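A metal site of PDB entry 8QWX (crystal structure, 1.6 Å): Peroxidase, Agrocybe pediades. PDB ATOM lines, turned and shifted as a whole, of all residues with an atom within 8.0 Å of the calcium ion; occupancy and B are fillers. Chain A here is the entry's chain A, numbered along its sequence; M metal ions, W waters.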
ATOM      1  N   LEU A  43      -4.600   4.550 -11.268  1.00  0.00           N
ATOM      2  CA  LEU A  43      -3.429   3.700 -11.188  1.00  0.00           C
ATOM      3  C   LEU A  43      -2.157   4.554 -11.230  1.00  0.00           C
ATOM      4  O   LEU A  43      -1.138   4.177 -10.647  1.00  0.00           O
ATOM      5  CB  LEU A  43      -3.516   2.671 -12.303  1.00  0.00           C
ATOM      6  CG  LEU A  43      -2.530   1.498 -12.244  1.00  0.00           C
ATOM      7  CD1 LEU A  43      -2.738   0.654 -11.002  1.00  0.00           C
ATOM      8  CD2 LEU A  43      -2.629   0.590 -13.497  1.00  0.00           C
ATOM      9  N   VAL A  44      -2.170   5.662 -12.001  1.00  0.00           N
ATOM     10  CA  VAL A  44      -1.050   6.558 -12.041  1.00  0.00           C
ATOM     11  C   VAL A  44      -0.645   6.944 -10.605  1.00  0.00           C
ATOM     12  O   VAL A  44       0.539   6.927 -10.232  1.00  0.00           O
ATOM     13  CB  VAL A  44      -1.386   7.823 -12.855  1.00  0.00           C
ATOM     14  CG1 VAL A  44      -0.392   8.942 -12.619  1.00  0.00           C
ATOM     15  CG2 VAL A  44      -1.510   7.497 -14.339  1.00  0.00           C
ATOM     16  N   PHE A  45      -1.620   7.403  -9.790  1.00  0.00           N
ATOM     17  CA  PHE A  45      -1.311   7.836  -8.444  1.00  0.00           C
ATOM     18  C   PHE A  45      -0.788   6.703  -7.563  1.00  0.00           C
ATOM     19  O   PHE A  45       0.209   6.859  -6.850  1.00  0.00           O
ATOM     20  CB  PHE A  45      -2.621   8.386  -7.868  1.00  0.00           C
ATOM     21  CG  PHE A  45      -2.557   8.906  -6.451  1.00  0.00           C
ATOM     22  CD1 PHE A  45      -1.617   9.853  -6.087  1.00  0.00           C
ATOM     23  CD2 PHE A  45      -3.465   8.457  -5.498  1.00  0.00           C
ATOM     24  CE1 PHE A  45      -1.608  10.363  -4.814  1.00  0.00           C
ATOM     25  CE2 PHE A  45      -3.407   8.973  -4.208  1.00  0.00           C
ATOM     26  CZ  PHE A  45      -2.446   9.902  -3.885  1.00  0.00           C
ATOM     27  N   HIS A  46      -1.475   5.558  -7.582  1.00  0.00           N
ATOM     28  CA  HIS A  46      -1.099   4.463  -6.713  1.00  0.00           C
ATOM     29  C   HIS A  46       0.284   3.902  -7.069  1.00  0.00           C
ATOM     30  O   HIS A  46       0.998   3.378  -6.168  1.00  0.00           O
ATOM     31  CB  HIS A  46      -2.217   3.420  -6.695  1.00  0.00           C
ATOM     32  CG  HIS A  46      -3.391   3.867  -5.903  1.00  0.00           C
ATOM     33  ND1 HIS A  46      -3.766   3.291  -4.705  1.00  0.00           N
ATOM     34  CD2 HIS A  46      -4.249   4.883  -6.132  1.00  0.00           C
ATOM     35  CE1 HIS A  46      -4.797   3.985  -4.228  1.00  0.00           C
ATOM     36  NE2 HIS A  46      -5.109   4.991  -5.046  1.00  0.00           N
ATOM     37  N   ASP A  47       0.632   3.922  -8.354  1.00  0.00           N
ATOM     38  CA  ASP A  47       1.988   3.559  -8.736  1.00  0.00           C
ATOM     39  C   ASP A  47       2.987   4.617  -8.268  1.00  0.00           C
ATOM     40  O   ASP A  47       3.965   4.278  -7.539  1.00  0.00           O
ATOM     41  CB  ASP A  47       2.184   3.355 -10.219  1.00  0.00           C
ATOM     42  CG  ASP A  47       3.480   2.625 -10.531  1.00  0.00           C
ATOM     43  OD1 ASP A  47       4.024   1.967  -9.564  1.00  0.00           O
ATOM     44  OD2 ASP A  47       3.944   2.745 -11.679  1.00  0.00           O
ATOM     45  N   ALA A  48       2.776   5.871  -8.678  1.00  0.00           N
ATOM     46  CA  ALA A  48       3.816   6.899  -8.640  1.00  0.00           C
ATOM     47  C   ALA A  48       4.038   7.467  -7.235  1.00  0.00           C
ATOM     48  O   ALA A  48       5.179   7.793  -6.892  1.00  0.00           O
ATOM     49  CB  ALA A  48       3.480   8.033  -9.602  1.00  0.00           C
ATOM     50  N   ILE A  49       2.980   7.668  -6.433  1.00  0.00           N
ATOM     51  CA  ILE A  49       3.134   8.394  -5.173  1.00  0.00           C
ATOM     52  C   ILE A  49       3.814   7.528  -4.122  1.00  0.00           C
ATOM     53  O   ILE A  49       4.207   8.018  -3.069  1.00  0.00           O
ATOM     54  CB  ILE A  49       1.766   8.883  -4.662  1.00  0.00           C
ATOM     55  CG1 ILE A  49       1.880  10.132  -3.787  1.00  0.00           C
ATOM     56  CG2 ILE A  49       1.014   7.769  -3.945  1.00  0.00           C
ATOM     57  CD1 ILE A  49       2.220  11.389  -4.553  1.00  0.00           C
ATOM     58  N   ALA A  50       3.961   6.226  -4.388  1.00  0.00           N
ATOM     59  CA  ALA A  50       4.478   5.297  -3.400  1.00  0.00           C
ATOM     60  C   ALA A  50       5.987   5.351  -3.385  1.00  0.00           C
ATOM     61  O   ALA A  50       6.692   4.411  -3.796  1.00  0.00           O
ATOM     62  CB  ALA A  50       3.927   3.923  -3.667  1.00  0.00           C
ATOM     63  N   ILE A  51       6.472   6.480  -2.901  1.00  0.00           N
ATOM     64  CA  ILE A  51       7.888   6.749  -2.792  1.00  0.00           C
ATOM     65  C   ILE A  51       8.000   7.775  -1.643  1.00  0.00           C
ATOM     66  O   ILE A  51       7.161   8.646  -1.465  1.00  0.00           O
ATOM     67  CB  ILE A  51       8.493   7.296  -4.100  1.00  0.00           C
ATOM     68  CG1 ILE A  51       9.949   7.723  -3.916  1.00  0.00           C
ATOM     69  CG2 ILE A  51       7.660   8.456  -4.633  1.00  0.00           C
ATOM     70  CD1 ILE A  51      10.674   7.934  -5.239  1.00  0.00           C
ATOM     71  N   GLY A  57      10.735   3.000  -1.704  1.00  0.00           N
ATOM     72  CA  GLY A  57       9.776   2.916  -2.780  1.00  0.00           C
ATOM     73  C   GLY A  57      10.362   3.528  -4.029  1.00  0.00           C
ATOM     74  O   GLY A  57      11.062   4.557  -3.968  1.00  0.00           O
ATOM     75  N   GLY A  58      10.047   2.941  -5.195  1.00  0.00           N
ATOM     76  CA  GLY A  58      10.645   3.436  -6.435  1.00  0.00           C
ATOM     77  C   GLY A  58       9.815   4.445  -7.226  1.00  0.00           C
ATOM     78  O   GLY A  58      10.270   4.916  -8.275  1.00  0.00           O
ATOM     79  N   GLY A  59       8.617   4.803  -6.768  1.00  0.00           N
ATOM     80  CA  GLY A  59       7.834   5.811  -7.446  1.00  0.00           C
ATOM     81  C   GLY A  59       7.156   5.271  -8.691  1.00  0.00           C
ATOM     82  O   GLY A  59       6.494   4.258  -8.656  1.00  0.00           O
ATOM     83  N   ALA A  60       7.299   6.011  -9.791  1.00  0.00           N
ATOM     84  CA  ALA A  60       6.585   5.678 -11.035  1.00  0.00           C
ATOM     85  C   ALA A  60       7.410   4.613 -11.747  1.00  0.00           C
ATOM     86  O   ALA A  60       8.127   4.937 -12.700  1.00  0.00           O
ATOM     87  CB  ALA A  60       6.419   6.923 -11.875  1.00  0.00           C
ATOM     88  N   ASP A  61       7.284   3.386 -11.257  1.00  0.00           N
ATOM     89  CA  ASP A  61       8.184   2.316 -11.633  1.00  0.00           C
ATOM     90  C   ASP A  61       7.443   1.051 -12.035  1.00  0.00           C
ATOM     91  O   ASP A  61       8.082   0.075 -12.387  1.00  0.00           O
ATOM     92  CB  ASP A  61       9.091   1.945 -10.472  1.00  0.00           C
ATOM     93  CG  ASP A  61       8.409   1.473  -9.192  1.00  0.00           C
ATOM     94  OD1 ASP A  61       7.155   1.544  -9.089  1.00  0.00           O
ATOM     95  OD2 ASP A  61       9.175   0.986  -8.291  1.00  0.00           O
ATOM     96  N   GLY A  62       6.113   1.057 -12.034  1.00  0.00           N
ATOM     97  CA  GLY A  62       5.340  -0.122 -12.381  1.00  0.00           C
ATOM     98  C   GLY A  62       5.202  -1.130 -11.250  1.00  0.00           C
ATOM     99  O   GLY A  62       4.671  -2.211 -11.467  1.00  0.00           O
ATOM    100  N   SER A  63       5.685  -0.788 -10.047  1.00  0.00           N
ATOM    101  CA  SER A  63       5.681  -1.755  -8.941  1.00  0.00           C
ATOM    102  C   SER A  63       4.282  -2.236  -8.600  1.00  0.00           C
ATOM    103  O   SER A  63       4.128  -3.373  -8.141  1.00  0.00           O
ATOM    104  CB  SER A  63       6.305  -1.181  -7.727  1.00  0.00           C
ATOM    105  OG  SER A  63       5.581  -0.049  -7.165  1.00  0.00           O
ATOM    106  N   ILE A  64       3.294  -1.356  -8.724  1.00  0.00           N
ATOM    107  CA  ILE A  64       1.941  -1.732  -8.329  1.00  0.00           C
ATOM    108  C   ILE A  64       1.455  -2.875  -9.217  1.00  0.00           C
ATOM    109  O   ILE A  64       0.575  -3.641  -8.767  1.00  0.00           O
ATOM    110  CB  ILE A  64       1.010  -0.496  -8.331  1.00  0.00           C
ATOM    111  CG1 ILE A  64      -0.329  -0.851  -7.662  1.00  0.00           C
ATOM    112  CG2 ILE A  64       0.783   0.054  -9.713  1.00  0.00           C
ATOM    113  CD1 ILE A  64      -0.856   0.149  -6.694  1.00  0.00           C
ATOM    114  N   ALA A  65       1.980  -3.007 -10.444  1.00  0.00           N
ATOM    115  CA  ALA A  65       1.585  -4.113 -11.303  1.00  0.00           C
ATOM    116  C   ALA A  65       2.487  -5.316 -11.085  1.00  0.00           C
ATOM    117  O   ALA A  65       2.038  -6.419 -10.770  1.00  0.00           O
ATOM    118  CB  ALA A  65       1.508  -3.644 -12.745  1.00  0.00           C
ATOM    119  N   PHE A  67       4.608  -6.066  -8.640  1.00  0.00           N
ATOM    120  CA  PHE A  67       4.638  -6.555  -7.272  1.00  0.00           C
ATOM    121  C   PHE A  67       3.248  -6.433  -6.661  1.00  0.00           C
ATOM    122  O   PHE A  67       3.104  -6.185  -5.464  1.00  0.00           O
ATOM    123  CB  PHE A  67       5.701  -5.787  -6.507  1.00  0.00           C
ATOM    124  CG  PHE A  67       7.075  -5.995  -7.104  1.00  0.00           C
ATOM    125  CD1 PHE A  67       7.660  -7.250  -7.090  1.00  0.00           C
ATOM    126  CD2 PHE A  67       7.803  -4.923  -7.597  1.00  0.00           C
ATOM    127  CE1 PHE A  67       8.928  -7.419  -7.636  1.00  0.00           C
ATOM    128  CE2 PHE A  67       9.043  -5.110  -8.148  1.00  0.00           C
ATOM    129  CZ  PHE A  67       9.622  -6.339  -8.160  1.00  0.00           C
ATOM    130  N   GLU A  71       1.682  -5.321  -3.055  1.00  0.00           N
ATOM    131  CA  GLU A  71       1.108  -3.999  -2.851  1.00  0.00           C
ATOM    132  C   GLU A  71      -0.420  -4.068  -2.735  1.00  0.00           C
ATOM    133  O   GLU A  71      -0.993  -3.200  -2.049  1.00  0.00           O
ATOM    134  CB  GLU A  71       1.529  -2.986  -3.934  1.00  0.00           C
ATOM    135  CG  GLU A  71       3.029  -2.724  -3.980  1.00  0.00           C
ATOM    136  CD  GLU A  71       3.441  -1.496  -4.804  1.00  0.00           C
ATOM    137  OE1 GLU A  71       2.596  -0.612  -5.058  1.00  0.00           O
ATOM    138  OE2 GLU A  71       4.630  -1.469  -5.222  1.00  0.00           O
ATOM    139  N   GLY A 101       6.251   0.742 -15.689  1.00  0.00           N
ATOM    140  CA  GLY A 101       6.114   2.100 -15.216  1.00  0.00           C
ATOM    141  C   GLY A 101       5.740   3.018 -16.368  1.00  0.00           C
ATOM    142  O   GLY A 101       4.896   3.904 -16.197  1.00  0.00           O
ATOM    143  N   ILE A 104       1.974   2.401 -17.340  1.00  0.00           N
ATOM    144  CA  ILE A 104       0.991   3.003 -16.447  1.00  0.00           C
ATOM    145  C   ILE A 104       0.876   4.505 -16.712  1.00  0.00           C
ATOM    146  O   ILE A 104      -0.249   5.080 -16.806  1.00  0.00           O
ATOM    147  CB  ILE A 104       1.296   2.661 -14.984  1.00  0.00           C
ATOM    148  CG1 ILE A 104       1.029   1.176 -14.733  1.00  0.00           C
ATOM    149  CG2 ILE A 104       0.546   3.582 -14.011  1.00  0.00           C
ATOM    150  CD1 ILE A 104       1.365   0.651 -13.318  1.00  0.00           C
ATOM    151  N   GLN A 105       2.003   5.190 -16.935  1.00  0.00           N
ATOM    152  CA  GLN A 105       1.902   6.619 -17.226  1.00  0.00           C
ATOM    153  C   GLN A 105       1.249   6.879 -18.580  1.00  0.00           C
ATOM    154  O   GLN A 105       0.474   7.842 -18.737  1.00  0.00           O
ATOM    155  CB  GLN A 105       3.280   7.277 -17.120  1.00  0.00           C
ATOM    156  CG  GLN A 105       3.852   7.184 -15.715  1.00  0.00           C
ATOM    157  CD  GLN A 105       2.954   7.789 -14.657  1.00  0.00           C
ATOM    158  OE1 GLN A 105       2.356   8.845 -14.889  1.00  0.00           O
ATOM    159  NE2 GLN A 105       2.791   7.138 -13.506  1.00  0.00           N
ATOM    160  N   PRO A 130      10.829  -2.089 -12.150  1.00  0.00           N
ATOM    161  CA  PRO A 130      10.872  -1.916 -10.695  1.00  0.00           C
ATOM    162  C   PRO A 130      11.743  -2.958  -9.997  1.00  0.00           C
ATOM    163  O   PRO A 130      11.853  -4.103 -10.461  1.00  0.00           O
ATOM    164  CB  PRO A 130       9.409  -2.047 -10.291  1.00  0.00           C
ATOM    165  CG  PRO A 130       8.847  -2.990 -11.327  1.00  0.00           C
ATOM    166  CD  PRO A 130       9.545  -2.651 -12.622  1.00  0.00           C
ATOM    167  N   ALA A 132      11.549  -3.479  -6.398  1.00  0.00           N
ATOM    168  CA  ALA A 132      10.834  -4.097  -5.288  1.00  0.00           C
ATOM    169  C   ALA A 132       9.471  -3.429  -5.123  1.00  0.00           C
ATOM    170  O   ALA A 132       9.253  -2.320  -5.616  1.00  0.00           O
ATOM    171  CB  ALA A 132      11.612  -3.998  -3.994  1.00  0.00           C
ATOM    172  N   ALA A 133       8.605  -4.087  -4.364  1.00  0.00           N
ATOM    173  CA  ALA A 133       7.366  -3.484  -3.919  1.00  0.00           C
ATOM    174  C   ALA A 133       7.666  -2.212  -3.164  1.00  0.00           C
ATOM    175  O   ALA A 133       8.662  -2.115  -2.448  1.00  0.00           O
ATOM    176  CB  ALA A 133       6.578  -4.445  -3.083  1.00  0.00           C
ATOM    177  N   ALA A 134       6.772  -1.239  -3.314  1.00  0.00           N
ATOM    178  CA  ALA A 134       6.716  -0.105  -2.434  1.00  0.00           C
ATOM    179  C   ALA A 134       6.509  -0.586  -0.999  1.00  0.00           C
ATOM    180  O   ALA A 134       5.779  -1.550  -0.722  1.00  0.00           O
ATOM    181  CB  ALA A 134       5.586   0.819  -2.813  1.00  0.00           C
ATOM    182  N   VAL A 139       0.753   5.453   0.219  1.00  0.00           N
ATOM    183  CA  VAL A 139      -0.358   6.014  -0.519  1.00  0.00           C
ATOM    184  C   VAL A 139      -1.299   6.692   0.468  1.00  0.00           C
ATOM    185  O   VAL A 139      -1.791   6.019   1.371  1.00  0.00           O
ATOM    186  CB  VAL A 139      -1.106   4.957  -1.343  1.00  0.00           C
ATOM    187  CG1 VAL A 139      -2.240   5.580  -2.117  1.00  0.00           C
ATOM    188  CG2 VAL A 139      -0.195   4.239  -2.337  1.00  0.00           C
ATOM    189  N   LEU A 270       8.254  10.691 -10.677  1.00  0.00           N
ATOM    190  CA  LEU A 270       8.663  10.392  -9.315  1.00  0.00           C
ATOM    191  C   LEU A 270       9.548   9.163  -9.307  1.00  0.00           C
ATOM    192  O   LEU A 270       9.220   8.183  -9.945  1.00  0.00           O
ATOM    193  CB  LEU A 270       7.461  10.226  -8.394  1.00  0.00           C
ATOM    194  CG  LEU A 270       6.697  11.503  -8.073  1.00  0.00           C
ATOM    195  CD1 LEU A 270       5.444  11.154  -7.334  1.00  0.00           C
ATOM    196  CD2 LEU A 270       7.556  12.449  -7.259  1.00  0.00           C
HETATM  197 CA    CA M   1       5.348   2.312  -7.728  1.00  0.00          CA
HETATM  198  O   HOH W   1       6.675   2.544  -5.729  1.00  0.00           O
HETATM  199  O   HOH W   2       3.453   1.631  -6.305  1.00  0.00           O
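The calcium ion is bound by the side-chain carboxylate (OD1) of Asp 47 (2.3 Å), the side-chain carboxylate (OD1) of Asp 61 (2.4 Å), water W1 (2.4 Å), the backbone carbonyl oxygen (O) of Asp 47 (2.4 Å), the side-chain hydroxyl (OG) of Ser 63 (2.4 Å), the backbone carbonyl oxygen (O) of Gly 59 (2.4 Å) and water W2 (2.5 Å).
The calcium ion has seven donor atoms within binding distance.
Within 4 Å of the calcium ion: Asp 47, Gly 59, Asp 61 and Ser 63.
The nearest printed residue that does not touch the calcium ion is Ile 64 (4.3 Å).
The side-chain carboxylate (OD2) of Asp 47 is in hydrogen-bond range of the backbone NH (N) of Gly 62 (2.8 Å).
The side-chain hydroxyl (OG) of Ser 63 sits close to the side-chain carboxylate (OE2) of Glu 71 (2.6 Å).
Water W2 bridges OE1 of Glu 71 (2.7 Å) and O of His 46 (3.0 Å).
Water W1 lies within hydrogen-bond range of O of Ala 50 (2.7 Å), N of Gly 59 (3.2 Å) and N of Gly 58 (3.4 Å).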
